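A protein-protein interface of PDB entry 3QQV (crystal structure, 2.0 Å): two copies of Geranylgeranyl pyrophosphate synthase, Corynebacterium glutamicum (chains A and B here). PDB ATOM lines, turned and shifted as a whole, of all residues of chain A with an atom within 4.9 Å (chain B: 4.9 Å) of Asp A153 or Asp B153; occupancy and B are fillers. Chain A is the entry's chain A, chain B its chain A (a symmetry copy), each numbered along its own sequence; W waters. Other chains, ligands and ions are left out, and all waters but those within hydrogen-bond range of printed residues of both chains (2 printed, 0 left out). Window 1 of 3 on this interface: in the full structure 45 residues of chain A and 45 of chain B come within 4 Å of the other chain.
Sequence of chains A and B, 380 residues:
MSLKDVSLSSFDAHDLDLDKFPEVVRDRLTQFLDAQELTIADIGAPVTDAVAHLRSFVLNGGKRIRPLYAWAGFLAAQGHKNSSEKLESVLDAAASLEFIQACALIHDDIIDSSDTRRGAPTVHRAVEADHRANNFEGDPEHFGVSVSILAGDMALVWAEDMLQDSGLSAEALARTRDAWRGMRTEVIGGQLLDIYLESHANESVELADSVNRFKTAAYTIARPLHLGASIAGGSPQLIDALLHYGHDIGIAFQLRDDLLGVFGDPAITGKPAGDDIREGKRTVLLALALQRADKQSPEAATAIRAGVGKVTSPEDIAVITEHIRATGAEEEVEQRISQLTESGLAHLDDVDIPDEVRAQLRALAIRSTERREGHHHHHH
ND1 of His A107 lies within hydrogen-bond range of OD2 of Asp B153 (2.7 Å).
OD2 of Asp A153 lies within hydrogen-bond range of ND1 of His B107 (2.7 Å).
A ring nitrogen (NE2) of His A107 sits at hydrogen-bond distance from the backbone carbonyl oxygen (O) of Ile A149, 2.8 Å away.
A ring nitrogen (NE2) of His B107 is in hydrogen-bond range of the backbone carbonyl oxygen of Ile B149, 2.8 Å away.
His A107 touches Ile B149 (ND1 to CG2, 3.4 Å).
Ile A149 touches His B107 (CG2 to ND1, 3.4 Å).
Leu B156 touches Asp A153.
Leu A156 touches Asp B153.
CD1 of Leu A156 touches CG2 of Val B157, 3.8 Å away.
Val A157 touches Leu B156 (CG2 to CD1, 3.8 Å).
Val A157 touches Ile B188 (CG2 to CD1, 3.8 Å).
Ile A188 touches Leu B150.
Asp B153 touches Ile A188 (O to CD1, 3.7 Å).
CD1 of Ile A188 touches CG2 of Val B157, at 3.8 Å.
Printed residues of chain B within 4 Å of Leu A150: Ile B188 (3.4 Å).
Gly B152 touches none of the printed residues of chain A.
Of chain A, only His A107 (2.7 Å), Asp A153 (3.5 Å), Leu A156 (3.9 Å) and Ile A188 (3.7 Å) come within 4 Å of Asp B153.
Of the printed residues of chain A, Leu B156 touches Asp A153 (3.9 Å), Leu A156 (3.9 Å) and Val A157 (3.8 Å).
Of the printed residues of chain A, Val B157 touches Leu A156 (3.8 Å) and Ile A188 (3.8 Å).
The nearest residue of chain B that does not touch Asp A153 is Cys B103 (4.1 Å).
Printed residues of chain A that touch a printed residue of chain B: His A107, Ile A149, Leu A150, Asp A153, Met A154, Leu A156, Val A157 and Ile A188.
Hydrophobic or aromatic side chains of chain A within 4 Å of the printed part of chain B: His A107, Ile A149, Met A154, Leu A156, Val A157 and Ile A188.
Of the 12 printed residues of chain B, 8 touch a printed residue of chain A.
Hydrophobic or aromatic side chains of chain B that line the printed part of chain A: His B107, Ile B149, Met B154, Leu B156, Val B157 and Ile B188.
Among the printed residues, no Asp or Glu carboxylate lies within 4 Å of a Lys or Arg side-chain nitrogen of the other chain.
His A107 touches Asp B153, and with the chains exchanged Asp A153 touches His B107.
Ile B149 touches its own counterpart, Ile A149.
Leu A150 touches Ile B188, and with the chains exchanged Ile A188 touches Leu B150.
Asp A153 touches Leu B156, and with the chains exchanged Leu A156 touches Asp B153.
12 positions are printed for both chains.
Water W1 lies within hydrogen-bond range of the side-chain carboxylate of Asp A153 and the side-chain sulfur of Cys B103.
Water W2 lies within hydrogen-bond range of OD2 of Asp B153 (2.9 Å) and SG of Cys A103 (3.8 Å).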
ATOM      1  N   CYS A 103      -2.099  32.743 -34.175  1.00  0.00           N
ATOM      2  CA  CYS A 103      -1.172  31.990 -33.328  1.00  0.00           C
ATOM      3  C   CYS A 103       0.031  31.481 -34.111  1.00  0.00           C
ATOM      4  O   CYS A 103       1.174  31.754 -33.737  1.00  0.00           O
ATOM      5  CB  CYS A 103      -1.862  30.802 -32.649  1.00  0.00           C
ATOM      6  SG  CYS A 103      -0.671  29.801 -31.696  1.00  0.00           S
ATOM      7  N   HIS A 107       3.920  33.117 -33.806  1.00  0.00           N
ATOM      8  CA  HIS A 107       4.950  32.208 -33.304  1.00  0.00           C
ATOM      9  C   HIS A 107       5.963  31.827 -34.377  1.00  0.00           C
ATOM     10  O   HIS A 107       7.160  31.736 -34.099  1.00  0.00           O
ATOM     11  CB  HIS A 107       4.321  30.960 -32.689  1.00  0.00           C
ATOM     12  CG  HIS A 107       3.651  31.207 -31.373  1.00  0.00           C
ATOM     13  ND1 HIS A 107       3.135  30.191 -30.599  1.00  0.00           N
ATOM     14  CD2 HIS A 107       3.422  32.353 -30.690  1.00  0.00           C
ATOM     15  CE1 HIS A 107       2.613  30.702 -29.500  1.00  0.00           C
ATOM     16  NE2 HIS A 107       2.777  32.010 -29.529  1.00  0.00           N
ATOM     17  N   ILE A 149       4.808  35.452 -27.649  1.00  0.00           N
ATOM     18  CA  ILE A 149       4.520  34.077 -27.262  1.00  0.00           C
ATOM     19  C   ILE A 149       3.131  34.013 -26.610  1.00  0.00           C
ATOM     20  O   ILE A 149       2.290  33.218 -27.029  1.00  0.00           O
ATOM     21  CB  ILE A 149       5.621  33.474 -26.355  1.00  0.00           C
ATOM     22  CG1 ILE A 149       6.913  33.281 -27.153  1.00  0.00           C
ATOM     23  CG2 ILE A 149       5.198  32.121 -25.826  1.00  0.00           C
ATOM     24  CD1 ILE A 149       8.129  32.972 -26.307  1.00  0.00           C
ATOM     25  N   LEU A 150       2.885  34.898 -25.647  1.00  0.00           N
ATOM     26  CA  LEU A 150       1.602  34.970 -24.947  1.00  0.00           C
ATOM     27  C   LEU A 150       0.442  35.488 -25.809  1.00  0.00           C
ATOM     28  O   LEU A 150      -0.702  35.058 -25.632  1.00  0.00           O
ATOM     29  CB  LEU A 150       1.729  35.812 -23.666  1.00  0.00           C
ATOM     30  CG  LEU A 150       2.646  35.267 -22.565  1.00  0.00           C
ATOM     31  CD1 LEU A 150       2.880  36.317 -21.497  1.00  0.00           C
ATOM     32  CD2 LEU A 150       2.092  33.991 -21.942  1.00  0.00           C
ATOM     33  N   ALA A 151       0.738  36.410 -26.731  1.00  0.00           N
ATOM     34  CA  ALA A 151      -0.263  36.915 -27.668  1.00  0.00           C
ATOM     35  C   ALA A 151      -0.759  35.782 -28.560  1.00  0.00           C
ATOM     36  O   ALA A 151      -1.953  35.657 -28.791  1.00  0.00           O
ATOM     37  CB  ALA A 151       0.290  38.071 -28.508  1.00  0.00           C
ATOM     38  N   GLY A 152       0.169  34.954 -29.026  1.00  0.00           N
ATOM     39  CA  GLY A 152      -0.162  33.751 -29.787  1.00  0.00           C
ATOM     40  C   GLY A 152      -0.970  32.728 -28.999  1.00  0.00           C
ATOM     41  O   GLY A 152      -1.891  32.116 -29.540  1.00  0.00           O
ATOM     42  N   ASP A 153      -0.625  32.550 -27.721  1.00  0.00           N
ATOM     43  CA  ASP A 153      -1.335  31.619 -26.833  1.00  0.00           C
ATOM     44  C   ASP A 153      -2.784  32.055 -26.635  1.00  0.00           C
ATOM     45  O   ASP A 153      -3.702  31.232 -26.701  1.00  0.00           O
ATOM     46  CB  ASP A 153      -0.632  31.516 -25.476  1.00  0.00           C
ATOM     47  CG  ASP A 153       0.733  30.876 -25.569  1.00  0.00           C
ATOM     48  OD1 ASP A 153       1.086  30.349 -26.646  1.00  0.00           O
ATOM     49  OD2 ASP A 153       1.455  30.893 -24.551  1.00  0.00           O
ATOM     50  N   MET A 154      -2.968  33.355 -26.411  1.00  0.00           N
ATOM     51  CA  MET A 154      -4.287  33.969 -26.311  1.00  0.00           C
ATOM     52  C   MET A 154      -5.110  33.771 -27.587  1.00  0.00           C
ATOM     53  O   MET A 154      -6.297  33.465 -27.513  1.00  0.00           O
ATOM     54  CB  MET A 154      -4.150  35.454 -25.992  1.00  0.00           C
ATOM     55  CG  MET A 154      -5.431  36.130 -25.582  1.00  0.00           C
ATOM     56  SD  MET A 154      -6.064  35.525 -23.825  1.00  0.00           S
ATOM     57  CE  MET A 154      -5.212  36.881 -22.676  1.00  0.00           C
ATOM     58  N   ALA A 155      -4.466  33.924 -28.743  1.00  0.00           N
ATOM     59  CA  ALA A 155      -5.130  33.737 -30.033  1.00  0.00           C
ATOM     60  C   ALA A 155      -5.638  32.299 -30.176  1.00  0.00           C
ATOM     61  O   ALA A 155      -6.779  32.070 -30.565  1.00  0.00           O
ATOM     62  CB  ALA A 155      -4.171  34.073 -31.162  1.00  0.00           C
ATOM     63  N   LEU A 156      -4.782  31.339 -29.829  1.00  0.00           N
ATOM     64  CA  LEU A 156      -5.115  29.925 -29.898  1.00  0.00           C
ATOM     65  C   LEU A 156      -6.273  29.549 -28.954  1.00  0.00           C
ATOM     66  O   LEU A 156      -7.179  28.807 -29.322  1.00  0.00           O
ATOM     67  CB  LEU A 156      -3.865  29.081 -29.620  1.00  0.00           C
ATOM     68  CG  LEU A 156      -3.965  27.556 -29.700  1.00  0.00           C
ATOM     69  CD1 LEU A 156      -4.595  27.082 -31.019  1.00  0.00           C
ATOM     70  CD2 LEU A 156      -2.593  26.942 -29.501  1.00  0.00           C
ATOM     71  N   VAL A 157      -6.241  30.094 -27.749  1.00  0.00           N
ATOM     72  CA  VAL A 157      -7.308  29.924 -26.770  1.00  0.00           C
ATOM     73  C   VAL A 157      -8.624  30.568 -27.252  1.00  0.00           C
ATOM     74  O   VAL A 157      -9.725  30.038 -27.031  1.00  0.00           O
ATOM     75  CB  VAL A 157      -6.808  30.465 -25.395  1.00  0.00           C
ATOM     76  CG1 VAL A 157      -7.895  31.117 -24.591  1.00  0.00           C
ATOM     77  CG2 VAL A 157      -6.145  29.328 -24.619  1.00  0.00           C
ATOM     78  N   ILE A 188       0.787  22.266 -36.080  1.00  0.00           N
ATOM     79  CA  ILE A 188       1.882  22.391 -35.119  1.00  0.00           C
ATOM     80  C   ILE A 188       2.939  21.316 -35.389  1.00  0.00           C
ATOM     81  O   ILE A 188       4.135  21.596 -35.327  1.00  0.00           O
ATOM     82  CB  ILE A 188       1.363  22.363 -33.651  1.00  0.00           C
ATOM     83  CG1 ILE A 188       0.450  23.574 -33.402  1.00  0.00           C
ATOM     84  CG2 ILE A 188       2.524  22.376 -32.655  1.00  0.00           C
ATOM     85  CD1 ILE A 188      -0.413  23.446 -32.173  1.00  0.00           C
ATOM     86  N   CYS B 103       1.798  23.896 -21.129  1.00  0.00           N
ATOM     87  CA  CYS B 103       1.900  25.069 -21.999  1.00  0.00           C
ATOM     88  C   CYS B 103       2.432  26.286 -21.254  1.00  0.00           C
ATOM     89  O   CYS B 103       3.425  26.886 -21.674  1.00  0.00           O
ATOM     90  CB  CYS B 103       0.552  25.424 -22.633  1.00  0.00           C
ATOM     91  SG  CYS B 103       0.666  26.958 -23.614  1.00  0.00           S
ATOM     92  N   HIS B 107       6.340  27.834 -21.728  1.00  0.00           N
ATOM     93  CA  HIS B 107       6.421  29.196 -22.253  1.00  0.00           C
ATOM     94  C   HIS B 107       6.916  30.194 -21.214  1.00  0.00           C
ATOM     95  O   HIS B 107       7.696  31.092 -21.535  1.00  0.00           O
ATOM     96  CB  HIS B 107       5.075  29.638 -22.826  1.00  0.00           C
ATOM     97  CG  HIS B 107       4.721  28.973 -24.120  1.00  0.00           C
ATOM     98  ND1 HIS B 107       3.613  29.326 -24.858  1.00  0.00           N
ATOM     99  CD2 HIS B 107       5.334  27.984 -24.811  1.00  0.00           C
ATOM    100  CE1 HIS B 107       3.557  28.579 -25.945  1.00  0.00           C
ATOM    101  NE2 HIS B 107       4.590  27.760 -25.942  1.00  0.00           N
ATOM    102  N   ILE B 149       8.378  26.694 -27.948  1.00  0.00           N
ATOM    103  CA  ILE B 149       7.195  27.468 -28.304  1.00  0.00           C
ATOM    104  C   ILE B 149       6.135  26.532 -28.902  1.00  0.00           C
ATOM    105  O   ILE B 149       4.995  26.518 -28.441  1.00  0.00           O
ATOM    106  CB  ILE B 149       7.526  28.655 -29.242  1.00  0.00           C
ATOM    107  CG1 ILE B 149       8.342  29.710 -28.489  1.00  0.00           C
ATOM    108  CG2 ILE B 149       6.258  29.319 -29.734  1.00  0.00           C
ATOM    109  CD1 ILE B 149       8.962  30.768 -29.376  1.00  0.00           C
ATOM    110  N   LEU B 150       6.544  25.714 -29.869  1.00  0.00           N
ATOM    111  CA  LEU B 150       5.653  24.754 -30.522  1.00  0.00           C
ATOM    112  C   LEU B 150       5.220  23.585 -29.625  1.00  0.00           C
ATOM    113  O   LEU B 150       4.096  23.090 -29.752  1.00  0.00           O
ATOM    114  CB  LEU B 150       6.285  24.222 -31.819  1.00  0.00           C
ATOM    115  CG  LEU B 150       6.516  25.235 -32.945  1.00  0.00           C
ATOM    116  CD1 LEU B 150       7.378  24.633 -34.036  1.00  0.00           C
ATOM    117  CD2 LEU B 150       5.206  25.750 -33.527  1.00  0.00           C
ATOM    118  N   ALA B 151       6.110  23.147 -28.729  1.00  0.00           N
ATOM    119  CA  ALA B 151       5.784  22.101 -27.762  1.00  0.00           C
ATOM    120  C   ALA B 151       4.671  22.577 -26.836  1.00  0.00           C
ATOM    121  O   ALA B 151       3.740  21.834 -26.559  1.00  0.00           O
ATOM    122  CB  ALA B 151       7.019  21.675 -26.962  1.00  0.00           C
ATOM    123  N   GLY B 152       4.771  23.825 -26.392  1.00  0.00           N
ATOM    124  CA  GLY B 152       3.721  24.464 -25.601  1.00  0.00           C
ATOM    125  C   GLY B 152       2.400  24.617 -26.343  1.00  0.00           C
ATOM    126  O   GLY B 152       1.335  24.418 -25.759  1.00  0.00           O
ATOM    127  N   ASP B 153       2.474  24.966 -27.630  1.00  0.00           N
ATOM    128  CA  ASP B 153       1.282  25.121 -28.476  1.00  0.00           C
ATOM    129  C   ASP B 153       0.546  23.793 -28.627  1.00  0.00           C
ATOM    130  O   ASP B 153      -0.681  23.740 -28.514  1.00  0.00           O
ATOM    131  CB  ASP B 153       1.662  25.666 -29.857  1.00  0.00           C
ATOM    132  CG  ASP B 153       2.191  27.079 -29.805  1.00  0.00           C
ATOM    133  OD1 ASP B 153       2.114  27.719 -28.734  1.00  0.00           O
ATOM    134  OD2 ASP B 153       2.680  27.557 -30.850  1.00  0.00           O
ATOM    135  N   MET B 154       1.316  22.732 -28.864  1.00  0.00           N
ATOM    136  CA  MET B 154       0.802  21.369 -28.924  1.00  0.00           C
ATOM    137  C   MET B 154       0.123  20.954 -27.616  1.00  0.00           C
ATOM    138  O   MET B 154      -0.941  20.341 -27.640  1.00  0.00           O
ATOM    139  CB  MET B 154       1.926  20.399 -29.271  1.00  0.00           C
ATOM    140  CG  MET B 154       1.470  19.014 -29.642  1.00  0.00           C
ATOM    141  SD  MET B 154       0.529  18.977 -31.365  1.00  0.00           S
ATOM    142  CE  MET B 154       2.043  18.586 -32.565  1.00  0.00           C
ATOM    143  N   ALA B 155       0.733  21.313 -26.486  1.00  0.00           N
ATOM    144  CA  ALA B 155       0.176  21.002 -25.170  1.00  0.00           C
ATOM    145  C   ALA B 155      -1.187  21.676 -24.986  1.00  0.00           C
ATOM    146  O   ALA B 155      -2.147  21.047 -24.552  1.00  0.00           O
ATOM    147  CB  ALA B 155       1.138  21.450 -24.083  1.00  0.00           C
ATOM    148  N   LEU B 156      -1.261  22.954 -25.350  1.00  0.00           N
ATOM    149  CA  LEU B 156      -2.486  23.733 -25.247  1.00  0.00           C
ATOM    150  C   LEU B 156      -3.610  23.177 -26.142  1.00  0.00           C
ATOM    151  O   LEU B 156      -4.762  23.079 -25.729  1.00  0.00           O
ATOM    152  CB  LEU B 156      -2.194  25.206 -25.559  1.00  0.00           C
ATOM    153  CG  LEU B 156      -3.330  26.226 -25.452  1.00  0.00           C
ATOM    154  CD1 LEU B 156      -4.062  26.144 -24.103  1.00  0.00           C
ATOM    155  CD2 LEU B 156      -2.788  27.622 -25.693  1.00  0.00           C
ATOM    156  N   VAL B 157      -3.251  22.791 -27.355  1.00  0.00           N
ATOM    157  CA  VAL B 157      -4.167  22.151 -28.291  1.00  0.00           C
ATOM    158  C   VAL B 157      -4.637  20.778 -27.770  1.00  0.00           C
ATOM    159  O   VAL B 157      -5.802  20.383 -27.942  1.00  0.00           O
ATOM    160  CB  VAL B 157      -3.484  22.094 -29.692  1.00  0.00           C
ATOM    161  CG1 VAL B 157      -3.832  20.856 -30.465  1.00  0.00           C
ATOM    162  CG2 VAL B 157      -3.834  23.358 -30.474  1.00  0.00           C
ATOM    163  N   ILE B 188      -3.402  33.427 -19.174  1.00  0.00           N
ATOM    164  CA  ILE B 188      -2.570  34.089 -20.176  1.00  0.00           C
ATOM    165  C   ILE B 188      -2.558  35.601 -19.930  1.00  0.00           C
ATOM    166  O   ILE B 188      -1.511  36.237 -20.040  1.00  0.00           O
ATOM    167  CB  ILE B 188      -3.015  33.724 -21.624  1.00  0.00           C
ATOM    168  CG1 ILE B 188      -2.828  32.216 -21.857  1.00  0.00           C
ATOM    169  CG2 ILE B 188      -2.214  34.511 -22.663  1.00  0.00           C
ATOM    170  CD1 ILE B 188      -3.579  31.686 -23.051  1.00  0.00           C
HETATM  171  O   HOH W   1       1.084  30.199 -21.755  1.00  0.00           O
HETATM  172  O   HOH W   2       1.826  27.750 -33.619  1.00  0.00           O
